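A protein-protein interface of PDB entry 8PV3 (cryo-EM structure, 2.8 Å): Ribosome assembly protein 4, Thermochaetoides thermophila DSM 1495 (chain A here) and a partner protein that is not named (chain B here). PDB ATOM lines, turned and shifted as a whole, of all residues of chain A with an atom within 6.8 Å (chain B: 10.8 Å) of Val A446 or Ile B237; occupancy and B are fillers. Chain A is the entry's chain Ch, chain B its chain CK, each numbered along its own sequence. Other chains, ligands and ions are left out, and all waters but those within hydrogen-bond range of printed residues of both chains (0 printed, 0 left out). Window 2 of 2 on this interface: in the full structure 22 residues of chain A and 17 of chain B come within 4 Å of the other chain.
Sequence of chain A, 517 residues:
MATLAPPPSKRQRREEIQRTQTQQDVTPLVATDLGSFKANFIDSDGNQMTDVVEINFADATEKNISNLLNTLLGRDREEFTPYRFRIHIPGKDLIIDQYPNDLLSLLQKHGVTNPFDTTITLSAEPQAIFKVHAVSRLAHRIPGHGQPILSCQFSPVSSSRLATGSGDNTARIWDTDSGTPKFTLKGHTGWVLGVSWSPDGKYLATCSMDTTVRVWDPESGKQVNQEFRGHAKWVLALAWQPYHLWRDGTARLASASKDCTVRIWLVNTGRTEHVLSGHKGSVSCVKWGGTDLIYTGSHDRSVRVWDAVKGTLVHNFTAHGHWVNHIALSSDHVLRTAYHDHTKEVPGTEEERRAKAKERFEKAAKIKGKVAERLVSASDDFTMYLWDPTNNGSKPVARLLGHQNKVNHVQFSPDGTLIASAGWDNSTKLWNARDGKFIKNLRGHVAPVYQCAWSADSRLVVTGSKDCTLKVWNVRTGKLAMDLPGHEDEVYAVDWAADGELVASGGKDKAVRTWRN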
ATOM      1  N   ASN A 426     -13.506 -25.913  -1.326  1.00  0.00           N
ATOM      2  CA  ASN A 426     -13.696 -24.466  -1.334  1.00  0.00           C
ATOM      3  C   ASN A 426     -13.611 -23.872  -2.735  1.00  0.00           C
ATOM      4  O   ASN A 426     -13.381 -22.669  -2.879  1.00  0.00           O
ATOM      5  CB  ASN A 426     -12.687 -23.752  -0.424  1.00  0.00           C
ATOM      6  CG  ASN A 426     -12.629 -24.346   0.965  1.00  0.00           C
ATOM      7  OD1 ASN A 426     -13.628 -24.813   1.496  1.00  0.00           O
ATOM      8  ND2 ASN A 426     -11.449 -24.322   1.565  1.00  0.00           N
ATOM      9  N   GLY A 444     -12.363 -18.073  -4.400  1.00  0.00           N
ATOM     10  CA  GLY A 444     -12.713 -17.003  -3.490  1.00  0.00           C
ATOM     11  C   GLY A 444     -13.340 -17.447  -2.184  1.00  0.00           C
ATOM     12  O   GLY A 444     -13.369 -16.675  -1.221  1.00  0.00           O
ATOM     13  N   HIS A 445     -13.816 -18.686  -2.120  1.00  0.00           N
ATOM     14  CA  HIS A 445     -14.565 -19.175  -0.968  1.00  0.00           C
ATOM     15  C   HIS A 445     -13.612 -19.806   0.036  1.00  0.00           C
ATOM     16  O   HIS A 445     -12.564 -20.337  -0.345  1.00  0.00           O
ATOM     17  CB  HIS A 445     -15.629 -20.187  -1.392  1.00  0.00           C
ATOM     18  CG  HIS A 445     -16.865 -19.567  -1.966  1.00  0.00           C
ATOM     19  ND1 HIS A 445     -17.694 -18.744  -1.236  1.00  0.00           N
ATOM     20  CD2 HIS A 445     -17.426 -19.670  -3.193  1.00  0.00           C
ATOM     21  CE1 HIS A 445     -18.705 -18.356  -1.992  1.00  0.00           C
ATOM     22  NE2 HIS A 445     -18.567 -18.906  -3.185  1.00  0.00           N
ATOM     23  N   VAL A 446     -13.974 -19.740   1.318  1.00  0.00           N
ATOM     24  CA  VAL A 446     -13.103 -20.270   2.363  1.00  0.00           C
ATOM     25  C   VAL A 446     -13.741 -21.480   3.031  1.00  0.00           C
ATOM     26  O   VAL A 446     -13.105 -22.177   3.831  1.00  0.00           O
ATOM     27  CB  VAL A 446     -12.763 -19.168   3.382  1.00  0.00           C
ATOM     28  CG1 VAL A 446     -11.868 -18.125   2.745  1.00  0.00           C
ATOM     29  CG2 VAL A 446     -14.032 -18.527   3.908  1.00  0.00           C
ATOM     30  N   ALA A 447     -14.999 -21.744   2.722  1.00  0.00           N
ATOM     31  CA  ALA A 447     -15.747 -22.902   3.177  1.00  0.00           C
ATOM     32  C   ALA A 447     -16.347 -23.621   1.974  1.00  0.00           C
ATOM     33  O   ALA A 447     -16.443 -23.045   0.885  1.00  0.00           O
ATOM     34  CB  ALA A 447     -16.841 -22.469   4.159  1.00  0.00           C
ATOM     35  N   PRO A 448     -16.706 -24.931   2.117  1.00  0.00           N
ATOM     36  CA  PRO A 448     -17.223 -25.699   0.971  1.00  0.00           C
ATOM     37  C   PRO A 448     -18.405 -25.083   0.239  1.00  0.00           C
ATOM     38  O   PRO A 448     -19.377 -24.641   0.856  1.00  0.00           O
ATOM     39  CB  PRO A 448     -17.630 -27.025   1.616  1.00  0.00           C
ATOM     40  CG  PRO A 448     -16.661 -27.204   2.701  1.00  0.00           C
ATOM     41  CD  PRO A 448     -16.302 -25.834   3.213  1.00  0.00           C
ATOM     42  N   VAL A 449     -18.318 -25.060  -1.088  1.00  0.00           N
ATOM     43  CA  VAL A 449     -19.332 -24.449  -1.937  1.00  0.00           C
ATOM     44  C   VAL A 449     -20.457 -25.455  -2.119  1.00  0.00           C
ATOM     45  O   VAL A 449     -20.226 -26.585  -2.562  1.00  0.00           O
ATOM     46  CB  VAL A 449     -18.746 -24.017  -3.289  1.00  0.00           C
ATOM     47  CG1 VAL A 449     -19.750 -23.185  -4.052  1.00  0.00           C
ATOM     48  CG2 VAL A 449     -17.471 -23.235  -3.073  1.00  0.00           C
ATOM     49  N   SER A 465     -22.029 -20.705  -0.768  1.00  0.00           N
ATOM     50  CA  SER A 465     -21.162 -21.600  -0.020  1.00  0.00           C
ATOM     51  C   SER A 465     -21.544 -21.653   1.451  1.00  0.00           C
ATOM     52  O   SER A 465     -22.482 -20.998   1.909  1.00  0.00           O
ATOM     53  CB  SER A 465     -19.695 -21.183  -0.155  1.00  0.00           C
ATOM     54  OG  SER A 465     -18.879 -21.911   0.743  1.00  0.00           O
ATOM     55  N   ASP A 467     -19.623 -20.579   3.806  1.00  0.00           N
ATOM     56  CA  ASP A 467     -19.072 -19.411   4.482  1.00  0.00           C
ATOM     57  C   ASP A 467     -20.025 -18.225   4.513  1.00  0.00           C
ATOM     58  O   ASP A 467     -19.552 -17.093   4.651  1.00  0.00           O
ATOM     59  CB  ASP A 467     -17.745 -18.988   3.836  1.00  0.00           C
ATOM     60  CG  ASP A 467     -17.877 -18.623   2.362  1.00  0.00           C
ATOM     61  OD1 ASP A 467     -18.981 -18.700   1.789  1.00  0.00           O
ATOM     62  OD2 ASP A 467     -16.849 -18.248   1.765  1.00  0.00           O
ATOM     63  N   THR A 469     -21.688 -16.797   2.166  1.00  0.00           N
ATOM     64  CA  THR A 469     -21.553 -15.847   1.074  1.00  0.00           C
ATOM     65  C   THR A 469     -22.008 -16.434  -0.255  1.00  0.00           C
ATOM     66  O   THR A 469     -21.918 -17.649  -0.508  1.00  0.00           O
ATOM     67  CB  THR A 469     -20.105 -15.350   0.922  1.00  0.00           C
ATOM     68  OG1 THR A 469     -19.281 -16.409   0.421  1.00  0.00           O
ATOM     69  CG2 THR A 469     -19.551 -14.838   2.239  1.00  0.00           C
ATOM     70  N   LYS A 471     -21.143 -15.625  -4.393  1.00  0.00           N
ATOM     71  CA  LYS A 471     -20.164 -14.968  -5.244  1.00  0.00           C
ATOM     72  C   LYS A 471     -20.568 -15.099  -6.701  1.00  0.00           C
ATOM     73  O   LYS A 471     -20.886 -16.193  -7.169  1.00  0.00           O
ATOM     74  CB  LYS A 471     -18.757 -15.537  -5.040  1.00  0.00           C
ATOM     75  CG  LYS A 471     -18.174 -15.250  -3.675  1.00  0.00           C
ATOM     76  CD  LYS A 471     -16.680 -15.424  -3.638  1.00  0.00           C
ATOM     77  CE  LYS A 471     -16.198 -15.422  -2.209  1.00  0.00           C
ATOM     78  NZ  LYS A 471     -16.779 -14.304  -1.431  1.00  0.00           N
ATOM     79  N   ASP A 483     -19.227  -9.845  -4.945  1.00  0.00           N
ATOM     80  CA  ASP A 483     -19.291 -10.533  -3.665  1.00  0.00           C
ATOM     81  C   ASP A 483     -20.569 -10.142  -2.937  1.00  0.00           C
ATOM     82  O   ASP A 483     -20.899  -8.959  -2.824  1.00  0.00           O
ATOM     83  CB  ASP A 483     -18.075 -10.197  -2.803  1.00  0.00           C
ATOM     84  CG  ASP A 483     -17.782 -11.262  -1.774  1.00  0.00           C
ATOM     85  OD1 ASP A 483     -17.200 -10.933  -0.719  1.00  0.00           O
ATOM     86  OD2 ASP A 483     -18.143 -12.430  -2.014  1.00  0.00           O
ATOM     87  N   LEU B 189     -20.031 -24.059  16.349  1.00  0.00           N
ATOM     88  CA  LEU B 189     -20.018 -25.059  15.290  1.00  0.00           C
ATOM     89  C   LEU B 189     -19.686 -26.453  15.800  1.00  0.00           C
ATOM     90  O   LEU B 189     -19.913 -27.425  15.072  1.00  0.00           O
ATOM     91  CB  LEU B 189     -19.019 -24.661  14.205  1.00  0.00           C
ATOM     92  CG  LEU B 189     -19.096 -23.219  13.713  1.00  0.00           C
ATOM     93  CD1 LEU B 189     -17.941 -22.918  12.773  1.00  0.00           C
ATOM     94  CD2 LEU B 189     -20.428 -22.963  13.034  1.00  0.00           C
ATOM     95  N   VAL B 193     -10.348 -27.952  15.357  1.00  0.00           N
ATOM     96  CA  VAL B 193      -9.347 -27.952  14.297  1.00  0.00           C
ATOM     97  C   VAL B 193      -8.011 -27.589  14.929  1.00  0.00           C
ATOM     98  O   VAL B 193      -7.947 -26.808  15.881  1.00  0.00           O
ATOM     99  CB  VAL B 193      -9.715 -26.962  13.158  1.00  0.00           C
ATOM    100  CG1 VAL B 193      -8.759 -27.072  11.977  1.00  0.00           C
ATOM    101  CG2 VAL B 193     -11.135 -27.175  12.682  1.00  0.00           C
ATOM    102  N   LEU B 195      -4.940 -25.421  14.732  1.00  0.00           N
ATOM    103  CA  LEU B 195      -4.683 -24.120  14.144  1.00  0.00           C
ATOM    104  C   LEU B 195      -3.319 -23.602  14.575  1.00  0.00           C
ATOM    105  O   LEU B 195      -2.854 -23.910  15.677  1.00  0.00           O
ATOM    106  CB  LEU B 195      -5.760 -23.109  14.559  1.00  0.00           C
ATOM    107  CG  LEU B 195      -7.208 -23.452  14.222  1.00  0.00           C
ATOM    108  CD1 LEU B 195      -8.131 -22.356  14.707  1.00  0.00           C
ATOM    109  CD2 LEU B 195      -7.364 -23.657  12.730  1.00  0.00           C
ATOM    110  N   LEU B 198      -0.718 -17.526  16.535  1.00  0.00           N
ATOM    111  CA  LEU B 198      -0.124 -16.299  16.026  1.00  0.00           C
ATOM    112  C   LEU B 198       0.667 -15.555  17.091  1.00  0.00           C
ATOM    113  O   LEU B 198       1.807 -15.160  16.838  1.00  0.00           O
ATOM    114  CB  LEU B 198      -1.200 -15.383  15.443  1.00  0.00           C
ATOM    115  CG  LEU B 198      -1.906 -15.876  14.182  1.00  0.00           C
ATOM    116  CD1 LEU B 198      -2.959 -14.880  13.742  1.00  0.00           C
ATOM    117  CD2 LEU B 198      -0.906 -16.123  13.074  1.00  0.00           C
ATOM    118  N   VAL B 223      -5.007 -16.951  17.418  1.00  0.00           N
ATOM    119  CA  VAL B 223      -4.927 -18.127  16.567  1.00  0.00           C
ATOM    120  C   VAL B 223      -5.362 -17.771  15.153  1.00  0.00           C
ATOM    121  O   VAL B 223      -6.133 -16.834  14.920  1.00  0.00           O
ATOM    122  CB  VAL B 223      -5.770 -19.297  17.112  1.00  0.00           C
ATOM    123  CG1 VAL B 223      -5.115 -19.884  18.342  1.00  0.00           C
ATOM    124  CG2 VAL B 223      -7.179 -18.838  17.421  1.00  0.00           C
ATOM    125  N   ASN B 224      -4.853 -18.554  14.204  1.00  0.00           N
ATOM    126  CA  ASN B 224      -5.139 -18.385  12.786  1.00  0.00           C
ATOM    127  C   ASN B 224      -6.380 -19.200  12.440  1.00  0.00           C
ATOM    128  O   ASN B 224      -6.349 -20.433  12.487  1.00  0.00           O
ATOM    129  CB  ASN B 224      -3.934 -18.829  11.957  1.00  0.00           C
ATOM    130  CG  ASN B 224      -3.992 -18.359  10.516  1.00  0.00           C
ATOM    131  OD1 ASN B 224      -5.049 -18.021   9.991  1.00  0.00           O
ATOM    132  ND2 ASN B 224      -2.837 -18.336   9.867  1.00  0.00           N
ATOM    133  N   VAL B 225      -7.457 -18.512  12.079  1.00  0.00           N
ATOM    134  CA  VAL B 225      -8.761 -19.134  11.889  1.00  0.00           C
ATOM    135  C   VAL B 225      -9.128 -19.223  10.408  1.00  0.00           C
ATOM    136  O   VAL B 225     -10.305 -19.169  10.060  1.00  0.00           O
ATOM    137  CB  VAL B 225      -9.845 -18.399  12.694  1.00  0.00           C
ATOM    138  CG1 VAL B 225      -9.637 -18.623  14.176  1.00  0.00           C
ATOM    139  CG2 VAL B 225      -9.827 -16.914  12.381  1.00  0.00           C
ATOM    140  N   SER B 226      -8.128 -19.343   9.531  1.00  0.00           N
ATOM    141  CA  SER B 226      -8.388 -19.418   8.096  1.00  0.00           C
ATOM    142  C   SER B 226      -9.142 -20.690   7.725  1.00  0.00           C
ATOM    143  O   SER B 226      -9.970 -20.685   6.807  1.00  0.00           O
ATOM    144  CB  SER B 226      -7.073 -19.342   7.324  1.00  0.00           C
ATOM    145  OG  SER B 226      -6.381 -18.143   7.610  1.00  0.00           O
ATOM    146  N   ASP B 227      -8.868 -21.789   8.427  1.00  0.00           N
ATOM    147  CA  ASP B 227      -9.475 -23.066   8.066  1.00  0.00           C
ATOM    148  C   ASP B 227     -10.913 -23.175   8.555  1.00  0.00           C
ATOM    149  O   ASP B 227     -11.627 -24.108   8.174  1.00  0.00           O
ATOM    150  CB  ASP B 227      -8.641 -24.216   8.624  1.00  0.00           C
ATOM    151  CG  ASP B 227      -7.203 -24.175   8.148  1.00  0.00           C
ATOM    152  OD1 ASP B 227      -6.294 -24.326   8.992  1.00  0.00           O
ATOM    153  OD2 ASP B 227      -6.980 -23.992   6.934  1.00  0.00           O
ATOM    154  N   LEU B 228     -11.354 -22.246   9.401  1.00  0.00           N
ATOM    155  CA  LEU B 228     -12.693 -22.323   9.970  1.00  0.00           C
ATOM    156  C   LEU B 228     -13.764 -21.693   9.090  1.00  0.00           C
ATOM    157  O   LEU B 228     -14.952 -21.899   9.357  1.00  0.00           O
ATOM    158  CB  LEU B 228     -12.706 -21.669  11.350  1.00  0.00           C
ATOM    159  CG  LEU B 228     -11.961 -22.473  12.411  1.00  0.00           C
ATOM    160  CD1 LEU B 228     -11.773 -21.656  13.660  1.00  0.00           C
ATOM    161  CD2 LEU B 228     -12.718 -23.748  12.726  1.00  0.00           C
ATOM    162  N   GLY B 229     -13.384 -20.948   8.058  1.00  0.00           N
ATOM    163  CA  GLY B 229     -14.355 -20.357   7.158  1.00  0.00           C
ATOM    164  C   GLY B 229     -15.185 -19.250   7.776  1.00  0.00           C
ATOM    165  O   GLY B 229     -16.414 -19.344   7.822  1.00  0.00           O
ATOM    166  N   ILE B 230     -14.526 -18.196   8.248  1.00  0.00           N
ATOM    167  CA  ILE B 230     -15.190 -17.081   8.911  1.00  0.00           C
ATOM    168  C   ILE B 230     -15.016 -15.840   8.049  1.00  0.00           C
ATOM    169  O   ILE B 230     -13.889 -15.472   7.700  1.00  0.00           O
ATOM    170  CB  ILE B 230     -14.623 -16.851  10.319  1.00  0.00           C
ATOM    171  CG1 ILE B 230     -14.673 -18.142  11.135  1.00  0.00           C
ATOM    172  CG2 ILE B 230     -15.386 -15.744  11.023  1.00  0.00           C
ATOM    173  CD1 ILE B 230     -14.036 -18.023  12.495  1.00  0.00           C
ATOM    174  N   VAL B 231     -16.126 -15.195   7.699  1.00  0.00           N
ATOM    175  CA  VAL B 231     -16.112 -13.944   6.952  1.00  0.00           C
ATOM    176  C   VAL B 231     -16.798 -12.877   7.792  1.00  0.00           C
ATOM    177  O   VAL B 231     -17.588 -13.189   8.692  1.00  0.00           O
ATOM    178  CB  VAL B 231     -16.794 -14.075   5.576  1.00  0.00           C
ATOM    179  CG1 VAL B 231     -16.169 -15.201   4.773  1.00  0.00           C
ATOM    180  CG2 VAL B 231     -18.286 -14.283   5.730  1.00  0.00           C
ATOM    181  N   THR B 232     -16.481 -11.619   7.510  1.00  0.00           N
ATOM    182  CA  THR B 232     -17.104 -10.512   8.213  1.00  0.00           C
ATOM    183  C   THR B 232     -18.345 -10.038   7.463  1.00  0.00           C
ATOM    184  O   THR B 232     -18.721 -10.577   6.419  1.00  0.00           O
ATOM    185  CB  THR B 232     -16.113  -9.365   8.388  1.00  0.00           C
ATOM    186  OG1 THR B 232     -15.896  -8.722   7.128  1.00  0.00           O
ATOM    187  CG2 THR B 232     -14.790  -9.886   8.915  1.00  0.00           C
ATOM    188  N   ALA B 233     -18.995  -9.013   8.020  1.00  0.00           N
ATOM    189  CA  ALA B 233     -20.191  -8.465   7.390  1.00  0.00           C
ATOM    190  C   ALA B 233     -19.863  -7.735   6.096  1.00  0.00           C
ATOM    191  O   ALA B 233     -20.714  -7.638   5.205  1.00  0.00           O
ATOM    192  CB  ALA B 233     -20.914  -7.533   8.360  1.00  0.00           C
ATOM    193  N   SER B 234     -18.644  -7.217   5.974  1.00  0.00           N
ATOM    194  CA  SER B 234     -18.208  -6.544   4.757  1.00  0.00           C
ATOM    195  C   SER B 234     -17.698  -7.508   3.697  1.00  0.00           C
ATOM    196  O   SER B 234     -17.333  -7.064   2.604  1.00  0.00           O
ATOM    197  CB  SER B 234     -17.118  -5.524   5.087  1.00  0.00           C
ATOM    198  OG  SER B 234     -17.619  -4.496   5.921  1.00  0.00           O
ATOM    199  N   GLY B 235     -17.664  -8.804   3.987  1.00  0.00           N
ATOM    200  CA  GLY B 235     -17.119  -9.779   3.068  1.00  0.00           C
ATOM    201  C   GLY B 235     -15.647 -10.067   3.240  1.00  0.00           C
ATOM    202  O   GLY B 235     -15.120 -10.938   2.538  1.00  0.00           O
ATOM    203  N   LYS B 236     -14.969  -9.366   4.142  1.00  0.00           N
ATOM    204  CA  LYS B 236     -13.560  -9.604   4.395  1.00  0.00           C
ATOM    205  C   LYS B 236     -13.376 -10.918   5.149  1.00  0.00           C
ATOM    206  O   LYS B 236     -14.259 -11.374   5.876  1.00  0.00           O
ATOM    207  CB  LYS B 236     -12.964  -8.441   5.186  1.00  0.00           C
ATOM    208  CG  LYS B 236     -13.127  -7.099   4.491  1.00  0.00           C
ATOM    209  CD  LYS B 236     -12.692  -5.943   5.372  1.00  0.00           C
ATOM    210  CE  LYS B 236     -11.185  -5.787   5.380  1.00  0.00           C
ATOM    211  NZ  LYS B 236     -10.674  -5.271   4.081  1.00  0.00           N
ATOM    212  N   ILE B 237     -12.214 -11.531   4.961  1.00  0.00           N
ATOM    213  CA  ILE B 237     -11.921 -12.828   5.561  1.00  0.00           C
ATOM    214  C   ILE B 237     -11.224 -12.595   6.894  1.00  0.00           C
ATOM    215  O   ILE B 237     -10.199 -11.908   6.958  1.00  0.00           O
ATOM    216  CB  ILE B 237     -11.052 -13.691   4.635  1.00  0.00           C
ATOM    217  CG1 ILE B 237     -11.617 -13.702   3.215  1.00  0.00           C
ATOM    218  CG2 ILE B 237     -10.961 -15.106   5.174  1.00  0.00           C
ATOM    219  CD1 ILE B 237     -13.003 -14.270   3.113  1.00  0.00           C
ATOM    220  N   ALA B 238     -11.774 -13.170   7.958  1.00  0.00           N
ATOM    221  CA  ALA B 238     -11.167 -13.084   9.281  1.00  0.00           C
ATOM    222  C   ALA B 238     -10.218 -14.259   9.460  1.00  0.00           C
ATOM    223  O   ALA B 238     -10.653 -15.413   9.507  1.00  0.00           O
ATOM    224  CB  ALA B 238     -12.241 -13.077  10.362  1.00  0.00           C
ATOM    225  N   TRP B 239      -8.920 -13.975   9.558  1.00  0.00           N
ATOM    226  CA  TRP B 239      -7.926 -15.020   9.734  1.00  0.00           C
ATOM    227  C   TRP B 239      -7.157 -14.915  11.042  1.00  0.00           C
ATOM    228  O   TRP B 239      -6.177 -15.643  11.221  1.00  0.00           O
ATOM    229  CB  TRP B 239      -6.940 -15.025   8.557  1.00  0.00           C
ATOM    230  CG  TRP B 239      -6.084 -13.806   8.446  1.00  0.00           C
ATOM    231  CD1 TRP B 239      -6.451 -12.592   7.953  1.00  0.00           C
ATOM    232  CD2 TRP B 239      -4.704 -13.693   8.807  1.00  0.00           C
ATOM    233  NE1 TRP B 239      -5.391 -11.724   7.998  1.00  0.00           N
ATOM    234  CE2 TRP B 239      -4.305 -12.376   8.516  1.00  0.00           C
ATOM    235  CE3 TRP B 239      -3.768 -14.575   9.353  1.00  0.00           C
ATOM    236  CZ2 TRP B 239      -3.013 -11.921   8.752  1.00  0.00           C
ATOM    237  CZ3 TRP B 239      -2.489 -14.122   9.587  1.00  0.00           C
ATOM    238  CH2 TRP B 239      -2.120 -12.808   9.286  1.00  0.00           C
ATOM    239  N   GLY B 240      -7.562 -14.035  11.950  1.00  0.00           N
ATOM    240  CA  GLY B 240      -6.963 -13.976  13.266  1.00  0.00           C
ATOM    241  C   GLY B 240      -8.005 -13.748  14.339  1.00  0.00           C
ATOM    242  O   GLY B 240      -8.767 -12.782  14.262  1.00  0.00           O
ATOM    243  N   ARG B 241      -8.062 -14.625  15.339  1.00  0.00           N
ATOM    244  CA  ARG B 241      -9.050 -14.492  16.402  1.00  0.00           C
ATOM    245  C   ARG B 241      -8.412 -14.835  17.739  1.00  0.00           C
ATOM    246  O   ARG B 241      -7.239 -15.195  17.815  1.00  0.00           O
ATOM    247  CB  ARG B 241     -10.279 -15.374  16.150  1.00  0.00           C
ATOM    248  CG  ARG B 241     -11.273 -14.788  15.164  1.00  0.00           C
ATOM    249  CD  ARG B 241     -12.618 -15.480  15.261  1.00  0.00           C
ATOM    250  NE  ARG B 241     -13.342 -15.094  16.465  1.00  0.00           N
ATOM    251  CZ  ARG B 241     -14.272 -14.150  16.508  1.00  0.00           C
ATOM    252  NH1 ARG B 241     -14.635 -13.489  15.423  1.00  0.00           N
ATOM    253  NH2 ARG B 241     -14.855 -13.867  17.669  1.00  0.00           N
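No residue of chain B comes within 4 Å of Asn A426. Of chain B, only Gly B229 (3.7 Å) and Ile B237 (3.98 Å) come within 4 Å of Val A446. Asp A467 touches one residue of chain B. Of the printed residues of chain B, Thr A469 touches Val B231 (3.8 Å). Printed residues of chain B within 4 Å of Asp A483: Gly B235. Val B193 touches none of the printed residues of chain A. Of the printed residues of chain A, Gly B229 touches Val A446 (3.7 Å). Printed residues of chain A within 4 Å of Val B231: Asp A467 (3.3 Å) and Thr A469 (3.8 Å). Ile B237 touches just one residue of chain A: Val A446 (3.98 Å). The nearest residue of chain A that does not touch Ile B237 is Gly A444 (5.0 Å).
OD2 of Asp A467 sits at hydrogen-bond distance from ND1 of His A445, at 3.2 Å. A ring nitrogen (ND1) of His A445 lies close to the side-chain hydroxyl (OG1) of Thr A469, 3.3 Å away. OD2 of Asp A467 is in hydrogen-bond range of N of Val A446 (3.3 Å). The side-chain hydroxyl (OG) of Ser A465 sits close to the side-chain carboxylate (OD1) of Asp A467, at 3.4 Å. The side-chain hydroxyl (OG1) of Thr A469 lies within hydrogen-bond range of the side-chain carboxylate (OD1) of Asp A467, 2.7 Å away. The side-chain carboxylate (OD1) of Asp A483 lies within salt-bridge range of the side-chain amino group (NZ) of Lys A471 (3.5 Å).
CA of Gly B229 touches CG2 of Val A446 (3.7 Å). Ile B237 touches Val A446. Val B231 touches Asp A467. CG2 of Val B231 touches CG2 of Thr A469, 3.8 Å away. O of Gly B235 touches OD1 of Asp A483 (3.9 Å).
Hydrophobic or aromatic side chains of chain A that line the printed part of chain B: Val A446. Among the printed residues, no Asp or Glu carboxylate lies within 4 Å of a Lys or Arg side-chain nitrogen of the other chain.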
